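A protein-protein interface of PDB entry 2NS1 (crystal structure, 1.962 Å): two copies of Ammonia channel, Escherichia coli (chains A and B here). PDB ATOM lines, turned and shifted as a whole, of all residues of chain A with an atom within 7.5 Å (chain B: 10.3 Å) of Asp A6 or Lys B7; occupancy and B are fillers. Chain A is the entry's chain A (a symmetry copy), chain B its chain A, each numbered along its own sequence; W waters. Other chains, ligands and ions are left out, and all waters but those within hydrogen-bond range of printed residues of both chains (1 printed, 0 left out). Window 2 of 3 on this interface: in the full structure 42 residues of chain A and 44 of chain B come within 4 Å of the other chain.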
ATOM      1  N   ALA A   3     -21.038 -24.993  -9.645  1.00  0.00           N
ATOM      2  CA  ALA A   3     -21.141 -26.413  -9.203  1.00  0.00           C
ATOM      3  C   ALA A   3     -19.969 -27.258  -9.728  1.00  0.00           C
ATOM      4  O   ALA A   3     -18.963 -27.431  -9.032  1.00  0.00           O
ATOM      5  CB  ALA A   3     -22.486 -27.004  -9.632  1.00  0.00           C
ATOM      6  N   VAL A   4     -20.110 -27.806 -10.935  1.00  0.00           N
ATOM      7  CA  VAL A   4     -18.980 -28.402 -11.651  1.00  0.00           C
ATOM      8  C   VAL A   4     -18.746 -27.572 -12.919  1.00  0.00           C
ATOM      9  O   VAL A   4     -19.691 -27.018 -13.517  1.00  0.00           O
ATOM     10  CB  VAL A   4     -19.208 -29.901 -11.968  1.00  0.00           C
ATOM     11  CG1 VAL A   4     -18.055 -30.482 -12.753  1.00  0.00           C
ATOM     12  CG2 VAL A   4     -19.385 -30.681 -10.676  1.00  0.00           C
ATOM     13  N   ALA A   5     -17.476 -27.439 -13.287  1.00  0.00           N
ATOM     14  CA  ALA A   5     -17.092 -26.700 -14.487  1.00  0.00           C
ATOM     15  C   ALA A   5     -17.296 -27.596 -15.691  1.00  0.00           C
ATOM     16  O   ALA A   5     -16.940 -28.788 -15.675  1.00  0.00           O
ATOM     17  CB  ALA A   5     -15.646 -26.247 -14.390  1.00  0.00           C
ATOM     18  N   ASP A   6     -17.870 -27.035 -16.741  1.00  0.00           N
ATOM     19  CA  ASP A   6     -17.998 -27.753 -18.001  1.00  0.00           C
ATOM     20  C   ASP A   6     -16.766 -27.406 -18.822  1.00  0.00           C
ATOM     21  O   ASP A   6     -16.516 -26.224 -19.074  1.00  0.00           O
ATOM     22  CB  ASP A   6     -19.295 -27.345 -18.696  1.00  0.00           C
ATOM     23  CG  ASP A   6     -19.559 -28.130 -19.971  1.00  0.00           C
ATOM     24  OD1 ASP A   6     -18.644 -28.264 -20.816  1.00  0.00           O
ATOM     25  OD2 ASP A   6     -20.687 -28.623 -20.143  1.00  0.00           O
ATOM     26  N   LYS A   7     -15.967 -28.403 -19.199  1.00  0.00           N
ATOM     27  CA  LYS A   7     -14.716 -28.141 -19.905  1.00  0.00           C
ATOM     28  C   LYS A   7     -14.972 -27.483 -21.260  1.00  0.00           C
ATOM     29  O   LYS A   7     -14.106 -26.791 -21.765  1.00  0.00           O
ATOM     30  CB  LYS A   7     -13.866 -29.425 -20.087  1.00  0.00           C
ATOM     31  CG  LYS A   7     -13.345 -29.974 -18.777  1.00  0.00           C
ATOM     32  CD  LYS A   7     -12.077 -30.805 -18.907  1.00  0.00           C
ATOM     33  CE  LYS A   7     -12.256 -32.064 -19.687  1.00  0.00           C
ATOM     34  NZ  LYS A   7     -11.060 -32.982 -19.488  1.00  0.00           N
ATOM     35  N   ALA A   8     -16.149 -27.705 -21.849  1.00  0.00           N
ATOM     36  CA  ALA A   8     -16.469 -27.107 -23.130  1.00  0.00           C
ATOM     37  C   ALA A   8     -16.630 -25.618 -22.936  1.00  0.00           C
ATOM     38  O   ALA A   8     -16.227 -24.827 -23.783  1.00  0.00           O
ATOM     39  CB  ALA A   8     -17.734 -27.702 -23.722  1.00  0.00           C
ATOM     40  N   ASP A   9     -17.244 -25.242 -21.827  1.00  0.00           N
ATOM     41  CA  ASP A   9     -17.447 -23.828 -21.502  1.00  0.00           C
ATOM     42  C   ASP A   9     -16.118 -23.178 -21.087  1.00  0.00           C
ATOM     43  O   ASP A   9     -15.867 -22.021 -21.410  1.00  0.00           O
ATOM     44  CB  ASP A   9     -18.467 -23.697 -20.397  1.00  0.00           C
ATOM     45  CG  ASP A   9     -19.862 -24.036 -20.859  1.00  0.00           C
ATOM     46  OD1 ASP A   9     -20.110 -23.999 -22.084  1.00  0.00           O
ATOM     47  OD2 ASP A   9     -20.706 -24.332 -19.985  1.00  0.00           O
ATOM     48  N   ASN A  10     -15.294 -23.920 -20.349  1.00  0.00           N
ATOM     49  CA  ASN A  10     -13.940 -23.448 -19.956  1.00  0.00           C
ATOM     50  C   ASN A  10     -13.141 -23.107 -21.214  1.00  0.00           C
ATOM     51  O   ASN A  10     -12.541 -22.061 -21.312  1.00  0.00           O
ATOM     52  CB  ASN A  10     -13.137 -24.507 -19.235  1.00  0.00           C
ATOM     53  CG  ASN A  10     -13.602 -24.750 -17.828  1.00  0.00           C
ATOM     54  OD1 ASN A  10     -14.242 -23.893 -17.210  1.00  0.00           O
ATOM     55  ND2 ASN A  10     -13.292 -25.949 -17.314  1.00  0.00           N
ATOM     56  N   ALA A  11     -13.107 -24.056 -22.133  1.00  0.00           N
ATOM     57  CA  ALA A  11     -12.422 -23.894 -23.411  1.00  0.00           C
ATOM     58  C   ALA A  11     -12.930 -22.676 -24.164  1.00  0.00           C
ATOM     59  O   ALA A  11     -12.156 -21.821 -24.564  1.00  0.00           O
ATOM     60  CB  ALA A  11     -12.607 -25.134 -24.244  1.00  0.00           C
ATOM     61  N   PHE A  12     -14.235 -22.596 -24.348  1.00  0.00           N
ATOM     62  CA  PHE A  12     -14.843 -21.495 -25.092  1.00  0.00           C
ATOM     63  C   PHE A  12     -14.491 -20.165 -24.446  1.00  0.00           C
ATOM     64  O   PHE A  12     -14.149 -19.194 -25.120  1.00  0.00           O
ATOM     65  CB  PHE A  12     -16.355 -21.708 -25.131  1.00  0.00           C
ATOM     66  CG  PHE A  12     -17.107 -20.644 -25.866  1.00  0.00           C
ATOM     67  CD1 PHE A  12     -16.853 -20.399 -27.205  1.00  0.00           C
ATOM     68  CD2 PHE A  12     -18.082 -19.890 -25.224  1.00  0.00           C
ATOM     69  CE1 PHE A  12     -17.550 -19.434 -27.891  1.00  0.00           C
ATOM     70  CE2 PHE A  12     -18.768 -18.901 -25.922  1.00  0.00           C
ATOM     71  CZ  PHE A  12     -18.498 -18.677 -27.237  1.00  0.00           C
ATOM     72  N   VAL A  91     -15.974 -22.546  -9.119  1.00  0.00           N
ATOM     73  CA  VAL A  91     -16.760 -22.447 -10.333  1.00  0.00           C
ATOM     74  C   VAL A  91     -17.656 -21.225 -10.219  1.00  0.00           C
ATOM     75  O   VAL A  91     -18.199 -20.955  -9.161  1.00  0.00           O
ATOM     76  CB  VAL A  91     -17.585 -23.702 -10.495  1.00  0.00           C
ATOM     77  CG1 VAL A  91     -18.617 -23.563 -11.605  1.00  0.00           C
ATOM     78  CG2 VAL A  91     -16.660 -24.852 -10.704  1.00  0.00           C
ATOM     79  N   GLY A  93     -20.761 -19.755 -12.546  1.00  0.00           N
ATOM     80  CA  GLY A  93     -21.587 -20.181 -13.679  1.00  0.00           C
ATOM     81  C   GLY A  93     -21.245 -21.617 -14.020  1.00  0.00           C
ATOM     82  O   GLY A  93     -21.427 -22.514 -13.193  1.00  0.00           O
ATOM     83  N   SER A  94     -20.750 -21.860 -15.235  1.00  0.00           N
ATOM     84  CA  SER A  94     -20.305 -23.200 -15.588  1.00  0.00           C
ATOM     85  C   SER A  94     -18.820 -23.283 -15.897  1.00  0.00           C
ATOM     86  O   SER A  94     -18.373 -24.271 -16.465  1.00  0.00           O
ATOM     87  CB  SER A  94     -21.119 -23.756 -16.760  1.00  0.00           C
ATOM     88  OG  SER A  94     -21.075 -22.907 -17.885  1.00  0.00           O
ATOM     89  N   ILE A  95     -18.057 -22.276 -15.479  1.00  0.00           N
ATOM     90  CA  ILE A  95     -16.609 -22.220 -15.736  1.00  0.00           C
ATOM     91  C   ILE A  95     -15.812 -21.983 -14.476  1.00  0.00           C
ATOM     92  O   ILE A  95     -16.354 -21.507 -13.486  1.00  0.00           O
ATOM     93  CB  ILE A  95     -16.253 -21.120 -16.769  1.00  0.00           C
ATOM     94  CG1 ILE A  95     -16.651 -19.711 -16.275  1.00  0.00           C
ATOM     95  CG2 ILE A  95     -16.946 -21.429 -18.072  1.00  0.00           C
ATOM     96  CD1 ILE A  95     -16.299 -18.583 -17.253  1.00  0.00           C
ATOM     97  N   TYR A  96     -14.527 -22.344 -14.500  1.00  0.00           N
ATOM     98  CA  TYR A  96     -13.650 -21.990 -13.389  1.00  0.00           C
ATOM     99  C   TYR A  96     -13.656 -20.474 -13.189  1.00  0.00           C
ATOM    100  O   TYR A  96     -13.625 -19.707 -14.135  1.00  0.00           O
ATOM    101  CB  TYR A  96     -12.248 -22.544 -13.571  1.00  0.00           C
ATOM    102  CG  TYR A  96     -12.219 -24.052 -13.416  1.00  0.00           C
ATOM    103  CD1 TYR A  96     -12.659 -24.644 -12.241  1.00  0.00           C
ATOM    104  CD2 TYR A  96     -11.836 -24.881 -14.468  1.00  0.00           C
ATOM    105  CE1 TYR A  96     -12.676 -26.013 -12.078  1.00  0.00           C
ATOM    106  CE2 TYR A  96     -11.841 -26.278 -14.323  1.00  0.00           C
ATOM    107  CZ  TYR A  96     -12.260 -26.826 -13.105  1.00  0.00           C
ATOM    108  OH  TYR A  96     -12.285 -28.177 -12.919  1.00  0.00           O
ATOM    109  N   ILE A  99     -11.274 -18.134 -14.896  1.00  0.00           N
ATOM    110  CA  ILE A  99     -11.560 -17.766 -16.290  1.00  0.00           C
ATOM    111  C   ILE A  99     -12.465 -16.559 -16.299  1.00  0.00           C
ATOM    112  O   ILE A  99     -12.299 -15.680 -17.102  1.00  0.00           O
ATOM    113  CB  ILE A  99     -12.162 -18.923 -17.089  1.00  0.00           C
ATOM    114  CG1 ILE A  99     -11.221 -20.147 -17.022  1.00  0.00           C
ATOM    115  CG2 ILE A  99     -12.413 -18.453 -18.514  1.00  0.00           C
ATOM    116  CD1 ILE A  99     -11.766 -21.467 -17.679  1.00  0.00           C
ATOM    117  N   GLY A 221     -21.360 -16.768 -21.430  1.00  0.00           N
ATOM    118  CA  GLY A 221     -20.707 -17.516 -20.370  1.00  0.00           C
ATOM    119  C   GLY A 221     -20.624 -19.011 -20.619  1.00  0.00           C
ATOM    120  O   GLY A 221     -20.146 -19.768 -19.777  1.00  0.00           O
ATOM    121  N   THR A 222     -21.075 -19.439 -21.782  1.00  0.00           N
ATOM    122  CA  THR A 222     -21.172 -20.859 -22.111  1.00  0.00           C
ATOM    123  C   THR A 222     -21.337 -20.971 -23.602  1.00  0.00           C
ATOM    124  O   THR A 222     -21.827 -20.036 -24.227  1.00  0.00           O
ATOM    125  CB  THR A 222     -22.387 -21.539 -21.371  1.00  0.00           C
ATOM    126  OG1 THR A 222     -22.656 -22.822 -21.944  1.00  0.00           O
ATOM    127  CG2 THR A 222     -23.633 -20.695 -21.468  1.00  0.00           C
ATOM    128  N   ALA A 223     -20.950 -22.106 -24.177  1.00  0.00           N
ATOM    129  CA  ALA A 223     -21.095 -22.327 -25.613  1.00  0.00           C
ATOM    130  C   ALA A 223     -22.488 -22.922 -25.888  1.00  0.00           C
ATOM    131  O   ALA A 223     -22.598 -24.056 -26.338  1.00  0.00           O
ATOM    132  CB  ALA A 223     -20.003 -23.265 -26.134  1.00  0.00           C
ATOM    133  N   ASN A 224     -23.535 -22.135 -25.625  1.00  0.00           N
ATOM    134  CA  ASN A 224     -24.918 -22.594 -25.733  1.00  0.00           C
ATOM    135  C   ASN A 224     -25.648 -21.857 -26.848  1.00  0.00           C
ATOM    136  O   ASN A 224     -25.026 -21.267 -27.743  1.00  0.00           O
ATOM    137  CB  ASN A 224     -25.627 -22.426 -24.376  1.00  0.00           C
ATOM    138  CG  ASN A 224     -25.865 -20.998 -24.019  1.00  0.00           C
ATOM    139  OD1 ASN A 224     -25.344 -20.086 -24.660  1.00  0.00           O
ATOM    140  ND2 ASN A 224     -26.604 -20.783 -22.957  1.00  0.00           N
ATOM    141  N   GLU A 225     -26.966 -21.868 -26.820  1.00  0.00           N
ATOM    142  CA  GLU A 225     -27.697 -21.297 -27.933  1.00  0.00           C
ATOM    143  C   GLU A 225     -27.719 -19.783 -27.887  1.00  0.00           C
ATOM    144  O   GLU A 225     -27.977 -19.152 -28.903  1.00  0.00           O
ATOM    145  CB  GLU A 225     -29.128 -21.863 -28.022  1.00  0.00           C
ATOM    146  CG  GLU A 225     -30.096 -21.360 -26.975  1.00  0.00           C
ATOM    147  CD  GLU A 225     -29.932 -21.999 -25.611  1.00  0.00           C
ATOM    148  OE1 GLU A 225     -29.068 -22.891 -25.428  1.00  0.00           O
ATOM    149  OE2 GLU A 225     -30.673 -21.574 -24.705  1.00  0.00           O
ATOM    150  N   VAL B   4     -29.224 -33.519 -29.815  1.00  0.00           N
ATOM    151  CA  VAL B   4     -28.765 -32.581 -28.789  1.00  0.00           C
ATOM    152  C   VAL B   4     -27.434 -31.987 -29.266  1.00  0.00           C
ATOM    153  O   VAL B   4     -26.638 -32.652 -29.959  1.00  0.00           O
ATOM    154  CB  VAL B   4     -28.642 -33.248 -27.396  1.00  0.00           C
ATOM    155  CG1 VAL B   4     -28.116 -32.277 -26.363  1.00  0.00           C
ATOM    156  CG2 VAL B   4     -29.997 -33.772 -26.953  1.00  0.00           C
ATOM    157  N   ALA B   5     -27.229 -30.714 -28.941  1.00  0.00           N
ATOM    158  CA  ALA B   5     -25.998 -30.014 -29.301  1.00  0.00           C
ATOM    159  C   ALA B   5     -24.921 -30.391 -28.304  1.00  0.00           C
ATOM    160  O   ALA B   5     -25.159 -30.436 -27.084  1.00  0.00           O
ATOM    161  CB  ALA B   5     -26.227 -28.514 -29.309  1.00  0.00           C
ATOM    162  N   ASP B   6     -23.732 -30.664 -28.813  1.00  0.00           N
ATOM    163  CA  ASP B   6     -22.585 -30.906 -27.950  1.00  0.00           C
ATOM    164  C   ASP B   6     -21.899 -29.564 -27.756  1.00  0.00           C
ATOM    165  O   ASP B   6     -21.514 -28.929 -28.743  1.00  0.00           O
ATOM    166  CB  ASP B   6     -21.666 -31.942 -28.595  1.00  0.00           C
ATOM    167  CG  ASP B   6     -20.494 -32.333 -27.708  1.00  0.00           C
ATOM    168  OD1 ASP B   6     -19.813 -31.440 -27.154  1.00  0.00           O
ATOM    169  OD2 ASP B   6     -20.243 -33.541 -27.553  1.00  0.00           O
ATOM    170  N   LYS B   7     -21.785 -29.095 -26.514  1.00  0.00           N
ATOM    171  CA  LYS B   7     -21.227 -27.771 -26.256  1.00  0.00           C
ATOM    172  C   LYS B   7     -19.768 -27.687 -26.703  1.00  0.00           C
ATOM    173  O   LYS B   7     -19.292 -26.605 -27.000  1.00  0.00           O
ATOM    174  CB  LYS B   7     -21.353 -27.362 -24.766  1.00  0.00           C
ATOM    175  CG  LYS B   7     -22.787 -27.157 -24.333  1.00  0.00           C
ATOM    176  CD  LYS B   7     -22.956 -26.214 -23.151  1.00  0.00           C
ATOM    177  CE  LYS B   7     -22.350 -26.719 -21.884  1.00  0.00           C
ATOM    178  NZ  LYS B   7     -22.844 -25.899 -20.701  1.00  0.00           N
ATOM    179  N   ALA B   8     -19.061 -28.819 -26.742  1.00  0.00           N
ATOM    180  CA  ALA B   8     -17.675 -28.821 -27.165  1.00  0.00           C
ATOM    181  C   ALA B   8     -17.627 -28.514 -28.643  1.00  0.00           C
ATOM    182  O   ALA B   8     -16.737 -27.810 -29.110  1.00  0.00           O
ATOM    183  CB  ALA B   8     -17.008 -30.154 -26.880  1.00  0.00           C
ATOM    184  N   ASP B   9     -18.574 -29.069 -29.381  1.00  0.00           N
ATOM    185  CA  ASP B   9     -18.658 -28.837 -30.825  1.00  0.00           C
ATOM    186  C   ASP B   9     -19.152 -27.411 -31.111  1.00  0.00           C
ATOM    187  O   ASP B   9     -18.702 -26.777 -32.060  1.00  0.00           O
ATOM    188  CB  ASP B   9     -19.581 -29.853 -31.454  1.00  0.00           C
ATOM    189  CG  ASP B   9     -18.987 -31.238 -31.472  1.00  0.00           C
ATOM    190  OD1 ASP B   9     -17.747 -31.356 -31.358  1.00  0.00           O
ATOM    191  OD2 ASP B   9     -19.769 -32.203 -31.606  1.00  0.00           O
ATOM    192  N   ASN B  10     -20.097 -26.933 -30.302  1.00  0.00           N
ATOM    193  CA  ASN B  10     -20.600 -25.538 -30.410  1.00  0.00           C
ATOM    194  C   ASN B  10     -19.427 -24.567 -30.260  1.00  0.00           C
ATOM    195  O   ASN B  10     -19.262 -23.659 -31.042  1.00  0.00           O
ATOM    196  CB  ASN B  10     -21.571 -25.178 -29.307  1.00  0.00           C
ATOM    197  CG  ASN B  10     -22.920 -25.814 -29.474  1.00  0.00           C
ATOM    198  OD1 ASN B  10     -23.313 -26.198 -30.581  1.00  0.00           O
ATOM    199  ND2 ASN B  10     -23.642 -25.947 -28.352  1.00  0.00           N
ATOM    200  N   ALA B  11     -18.670 -24.759 -29.194  1.00  0.00           N
ATOM    201  CA  ALA B  11     -17.488 -23.952 -28.909  1.00  0.00           C
ATOM    202  C   ALA B  11     -16.504 -23.979 -30.066  1.00  0.00           C
ATOM    203  O   ALA B  11     -16.093 -22.942 -30.562  1.00  0.00           O
ATOM    204  CB  ALA B  11     -16.828 -24.452 -27.652  1.00  0.00           C
ATOM    205  N   PHE B  12     -16.133 -25.170 -30.498  1.00  0.00           N
ATOM    206  CA  PHE B  12     -15.159 -25.330 -31.578  1.00  0.00           C
ATOM    207  C   PHE B  12     -15.647 -24.627 -32.835  1.00  0.00           C
ATOM    208  O   PHE B  12     -14.892 -23.938 -33.519  1.00  0.00           O
ATOM    209  CB  PHE B  12     -14.944 -26.822 -31.825  1.00  0.00           C
ATOM    210  CG  PHE B  12     -13.966 -27.130 -32.913  1.00  0.00           C
ATOM    211  CD1 PHE B  12     -12.653 -26.698 -32.823  1.00  0.00           C
ATOM    212  CD2 PHE B  12     -14.350 -27.865 -34.029  1.00  0.00           C
ATOM    213  CE1 PHE B  12     -11.744 -26.989 -33.812  1.00  0.00           C
ATOM    214  CE2 PHE B  12     -13.429 -28.137 -35.034  1.00  0.00           C
ATOM    215  CZ  PHE B  12     -12.144 -27.698 -34.924  1.00  0.00           C
ATOM    216  N   MET B  13     -16.928 -24.802 -33.148  1.00  0.00           N
ATOM    217  CA  MET B  13     -17.446 -24.304 -34.397  1.00  0.00           C
ATOM    218  C   MET B  13     -17.674 -22.774 -34.394  1.00  0.00           C
ATOM    219  O   MET B  13     -17.557 -22.126 -35.426  1.00  0.00           O
ATOM    220  CB  MET B  13     -18.721 -25.072 -34.773  1.00  0.00           C
ATOM    221  CG  MET B  13     -18.442 -26.525 -35.199  1.00  0.00           C
ATOM    222  SD  MET B  13     -17.274 -26.678 -36.575  1.00  0.00           S
ATOM    223  CE  MET B  13     -18.233 -25.866 -37.866  1.00  0.00           C
ATOM    224  N   MET B  14     -18.004 -22.195 -33.254  1.00  0.00           N
ATOM    225  CA  MET B  14     -18.050 -20.724 -33.154  1.00  0.00           C
ATOM    226  C   MET B  14     -16.642 -20.162 -33.343  1.00  0.00           C
ATOM    227  O   MET B  14     -16.465 -19.211 -34.091  1.00  0.00           O
ATOM    228  CB  MET B  14     -18.673 -20.273 -31.837  1.00  0.00           C
ATOM    229  CG  MET B  14     -20.214 -20.288 -31.902  1.00  0.00           C
ATOM    230  SD  MET B  14     -21.003 -19.706 -30.426  1.00  0.00           S
ATOM    231  CE  MET B  14     -20.691 -21.050 -29.313  1.00  0.00           C
ATOM    232  N   ILE B  15     -15.630 -20.781 -32.724  1.00  0.00           N
ATOM    233  CA  ILE B  15     -14.267 -20.258 -32.884  1.00  0.00           C
ATOM    234  C   ILE B  15     -13.787 -20.491 -34.298  1.00  0.00           C
ATOM    235  O   ILE B  15     -13.144 -19.626 -34.884  1.00  0.00           O
ATOM    236  CB  ILE B  15     -13.288 -20.844 -31.875  1.00  0.00           C
ATOM    237  CG1 ILE B  15     -13.730 -20.533 -30.435  1.00  0.00           C
ATOM    238  CG2 ILE B  15     -11.902 -20.286 -32.102  1.00  0.00           C
ATOM    239  CD1 ILE B  15     -14.001 -19.057 -30.166  1.00  0.00           C
ATOM    240  N   VAL B  91     -30.807 -28.091 -33.831  1.00  0.00           N
ATOM    241  CA  VAL B  91     -29.494 -28.699 -33.939  1.00  0.00           C
ATOM    242  C   VAL B  91     -29.305 -29.164 -35.373  1.00  0.00           C
ATOM    243  O   VAL B  91     -30.227 -29.681 -35.981  1.00  0.00           O
ATOM    244  CB  VAL B  91     -29.405 -29.864 -32.982  1.00  0.00           C
ATOM    245  CG1 VAL B  91     -28.154 -30.699 -33.220  1.00  0.00           C
ATOM    246  CG2 VAL B  91     -29.495 -29.339 -31.589  1.00  0.00           C
ATOM    247  N   GLY B  93     -26.384 -31.428 -37.258  1.00  0.00           N
ATOM    248  CA  GLY B  93     -25.222 -32.248 -36.902  1.00  0.00           C
ATOM    249  C   GLY B  93     -25.143 -32.354 -35.393  1.00  0.00           C
ATOM    250  O   GLY B  93     -26.061 -32.882 -34.757  1.00  0.00           O
ATOM    251  N   SER B  94     -24.057 -31.860 -34.797  1.00  0.00           N
ATOM    252  CA  SER B  94     -23.967 -31.838 -33.343  1.00  0.00           C
ATOM    253  C   SER B  94     -23.882 -30.436 -32.765  1.00  0.00           C
ATOM    254  O   SER B  94     -23.531 -30.281 -31.602  1.00  0.00           O
ATOM    255  CB  SER B  94     -22.789 -32.684 -32.854  1.00  0.00           C
ATOM    256  OG  SER B  94     -21.569 -32.276 -33.432  1.00  0.00           O
ATOM    257  N   ILE B  95     -24.249 -29.430 -33.554  1.00  0.00           N
ATOM    258  CA  ILE B  95     -24.188 -28.024 -33.125  1.00  0.00           C
ATOM    259  C   ILE B  95     -25.498 -27.303 -33.337  1.00  0.00           C
ATOM    260  O   ILE B  95     -26.323 -27.748 -34.125  1.00  0.00           O
ATOM    261  CB  ILE B  95     -23.065 -27.248 -33.861  1.00  0.00           C
ATOM    262  CG1 ILE B  95     -23.288 -27.217 -35.391  1.00  0.00           C
ATOM    263  CG2 ILE B  95     -21.739 -27.891 -33.543  1.00  0.00           C
ATOM    264  CD1 ILE B  95     -22.214 -26.442 -36.163  1.00  0.00           C
ATOM    265  N   TYR B  96     -25.704 -26.204 -32.610  1.00  0.00           N
ATOM    266  CA  TYR B  96     -26.861 -25.357 -32.880  1.00  0.00           C
ATOM    267  C   TYR B  96     -26.835 -24.896 -34.337  1.00  0.00           C
ATOM    268  O   TYR B  96     -25.801 -24.541 -34.874  1.00  0.00           O
ATOM    269  CB  TYR B  96     -26.956 -24.194 -31.906  1.00  0.00           C
ATOM    270  CG  TYR B  96     -27.332 -24.662 -30.513  1.00  0.00           C
ATOM    271  CD1 TYR B  96     -28.509 -25.366 -30.304  1.00  0.00           C
ATOM    272  CD2 TYR B  96     -26.474 -24.475 -29.431  1.00  0.00           C
ATOM    273  CE1 TYR B  96     -28.866 -25.832 -29.056  1.00  0.00           C
ATOM    274  CE2 TYR B  96     -26.820 -24.937 -28.151  1.00  0.00           C
ATOM    275  CZ  TYR B  96     -28.035 -25.611 -27.984  1.00  0.00           C
ATOM    276  OH  TYR B  96     -28.410 -26.082 -26.761  1.00  0.00           O
ATOM    277  N   ILE B  99     -25.150 -21.757 -35.504  1.00  0.00           N
ATOM    278  CA  ILE B  99     -23.691 -21.791 -35.682  1.00  0.00           C
ATOM    279  C   ILE B  99     -23.382 -22.259 -37.081  1.00  0.00           C
ATOM    280  O   ILE B  99     -22.490 -21.753 -37.709  1.00  0.00           O
ATOM    281  CB  ILE B  99     -22.994 -22.660 -34.633  1.00  0.00           C
ATOM    282  CG1 ILE B  99     -23.368 -22.167 -33.218  1.00  0.00           C
ATOM    283  CG2 ILE B  99     -21.494 -22.626 -34.890  1.00  0.00           C
ATOM    284  CD1 ILE B  99     -22.841 -23.047 -32.026  1.00  0.00           C
ATOM    285  N   GLY B 221     -17.162 -30.286 -38.625  1.00  0.00           N
ATOM    286  CA  GLY B 221     -18.399 -29.998 -37.920  1.00  0.00           C
ATOM    287  C   GLY B 221     -18.385 -30.374 -36.450  1.00  0.00           C
ATOM    288  O   GLY B 221     -19.385 -30.237 -35.750  1.00  0.00           O
ATOM    289  N   THR B 222     -17.245 -30.838 -35.973  1.00  0.00           N
ATOM    290  CA  THR B 222     -17.117 -31.354 -34.613  1.00  0.00           C
ATOM    291  C   THR B 222     -15.649 -31.420 -34.288  1.00  0.00           C
ATOM    292  O   THR B 222     -14.834 -31.530 -35.196  1.00  0.00           O
ATOM    293  CB  THR B 222     -17.774 -32.781 -34.475  1.00  0.00           C
ATOM    294  OG1 THR B 222     -17.362 -33.396 -33.250  1.00  0.00           O
ATOM    295  CG2 THR B 222     -17.385 -33.681 -35.622  1.00  0.00           C
ATOM    296  N   ALA B 223     -15.305 -31.368 -33.004  1.00  0.00           N
ATOM    297  CA  ALA B 223     -13.910 -31.452 -32.580  1.00  0.00           C
ATOM    298  C   ALA B 223     -13.536 -32.934 -32.391  1.00  0.00           C
ATOM    299  O   ALA B 223     -13.245 -33.361 -31.280  1.00  0.00           O
ATOM    300  CB  ALA B 223     -13.686 -30.676 -31.279  1.00  0.00           C
HETATM  301  O   HOH W   1     -24.862 -24.143 -20.885  1.00  0.00           O
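N of Asp A9 lies within hydrogen-bond range of OD1 of Asp A6 (3.5 Å).
The side-chain carboxylate of Asp A9 is in hydrogen-bond range of the backbone NH of Ala A223.
OD2 of Asp A9 lies within hydrogen-bond range of OG of Ser A94 (2.6 Å).
The backbone carbonyl oxygen (O) of Ser A94 lies within hydrogen-bond range of the backbone NH (N) of Asp A6 (2.8 Å).
OD1 of Asp A6 sits at hydrogen-bond distance from N of Ala A8.
OD1 of Asp A9 is in hydrogen-bond range of OG1 of Thr A222 (2.8 Å).
Of the 21 printed residues of chain B, 6 touch a printed residue of chain A.
Hydrophobic or aromatic side chains of chain B within 4 Å of the printed part of chain A: Ala B11, Met B14 and Tyr B96.
Of the 21 printed residues of chain A, 8 touch a printed residue of chain B.
Among the printed residues, 14 pairs touch across the chains.
Asp A6 touches Lys B7, but with the chains exchanged Lys A7 does not touch Asp B6 (8.6 Å).
Ala A8 touches Lys B7, but with the chains exchanged Lys A7 does not touch Ala B8 (6.5 Å).
Ala B8 touches its own counterpart, Ala A8.
Ala A223 touches Lys B7, but with the chains exchanged Lys A7 does not touch Ala B223 (10.3 Å).
Among the printed residues, pairs that only touch across the chains: Ala A8 with Lys B7 (3.6 Å), Ala A8 with Ala B8 (3.5 Å), Ala A8 with Ala B11 (3.9 Å), Phe A12 with Ala B11 (3.8 Å), Phe A12 with Met B14 (3.8 Å), Ala A223 with Lys B7 (3.5 Å), Ala A223 with Ala B11 (3.7 Å), Ala A223 with Met B14 (3.9 Å), Asn A224 with Tyr B96 (3.5 Å) and Glu A225 with Tyr B96 (3.3 Å).
Water W1 lies within hydrogen-bond range of NZ of Lys B7 and OG1 of Thr A222.
Of the printed residues of chain A, Lys B7 touches Asp A6 (3.1 Å), Ala A8 (3.6 Å), Asp A9 (2.7 Å), Thr A222 (3.3 Å) and Ala A223 (3.5 Å).
No residue of chain B comes within 4 Å of Ala A5.
Of chain B, only Lys B7 (3.6 Å), Ala B8 (3.5 Å) and Ala B11 (3.9 Å) come within 4 Å of Ala A8.
Asp A9 touches just one residue of chain B: Lys B7 (2.7 Å).
No residue of chain B comes within 4 Å of Asn A10.
Ala A223 touches just these residues of chain B: Lys B7, Asn B10, Ala B11 and Met B14.
Printed residues of chain A within 4 Å of Tyr B96: Asn A224 and Glu A225.
Printed residues of chain B within 4 Å of Asn A224: Tyr B96 (3.5 Å).
Of the printed residues of chain A, Met B14 touches Phe A12 and Ala A223.
Of the printed residues of chain B, Glu A225 touches Tyr B96.
Gly A93 touches none of the printed residues of chain B.
Asp B6 touches none of the printed residues of chain A.
The nearest residue of chain A that does not touch Lys B7 is Ser A94 (4.5 Å).
The side-chain amino group (NZ) of Lys B7 is in salt-bridge range of the side-chain carboxylate (OD2) of Asp A9 (2.7 Å).
The side-chain amino group (NZ) of Lys B7 is in hydrogen-bond range of the side-chain hydroxyl (OG1) of Thr A222, 3.3 Å away.
The side-chain amide nitrogen (ND2) of Asn B10 is in hydrogen-bond range of the backbone carbonyl oxygen (O) of Ala A223 (3.0 Å).
NZ of Lys B7 is in salt-bridge range of OD2 of Asp A6 (3.5 Å).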
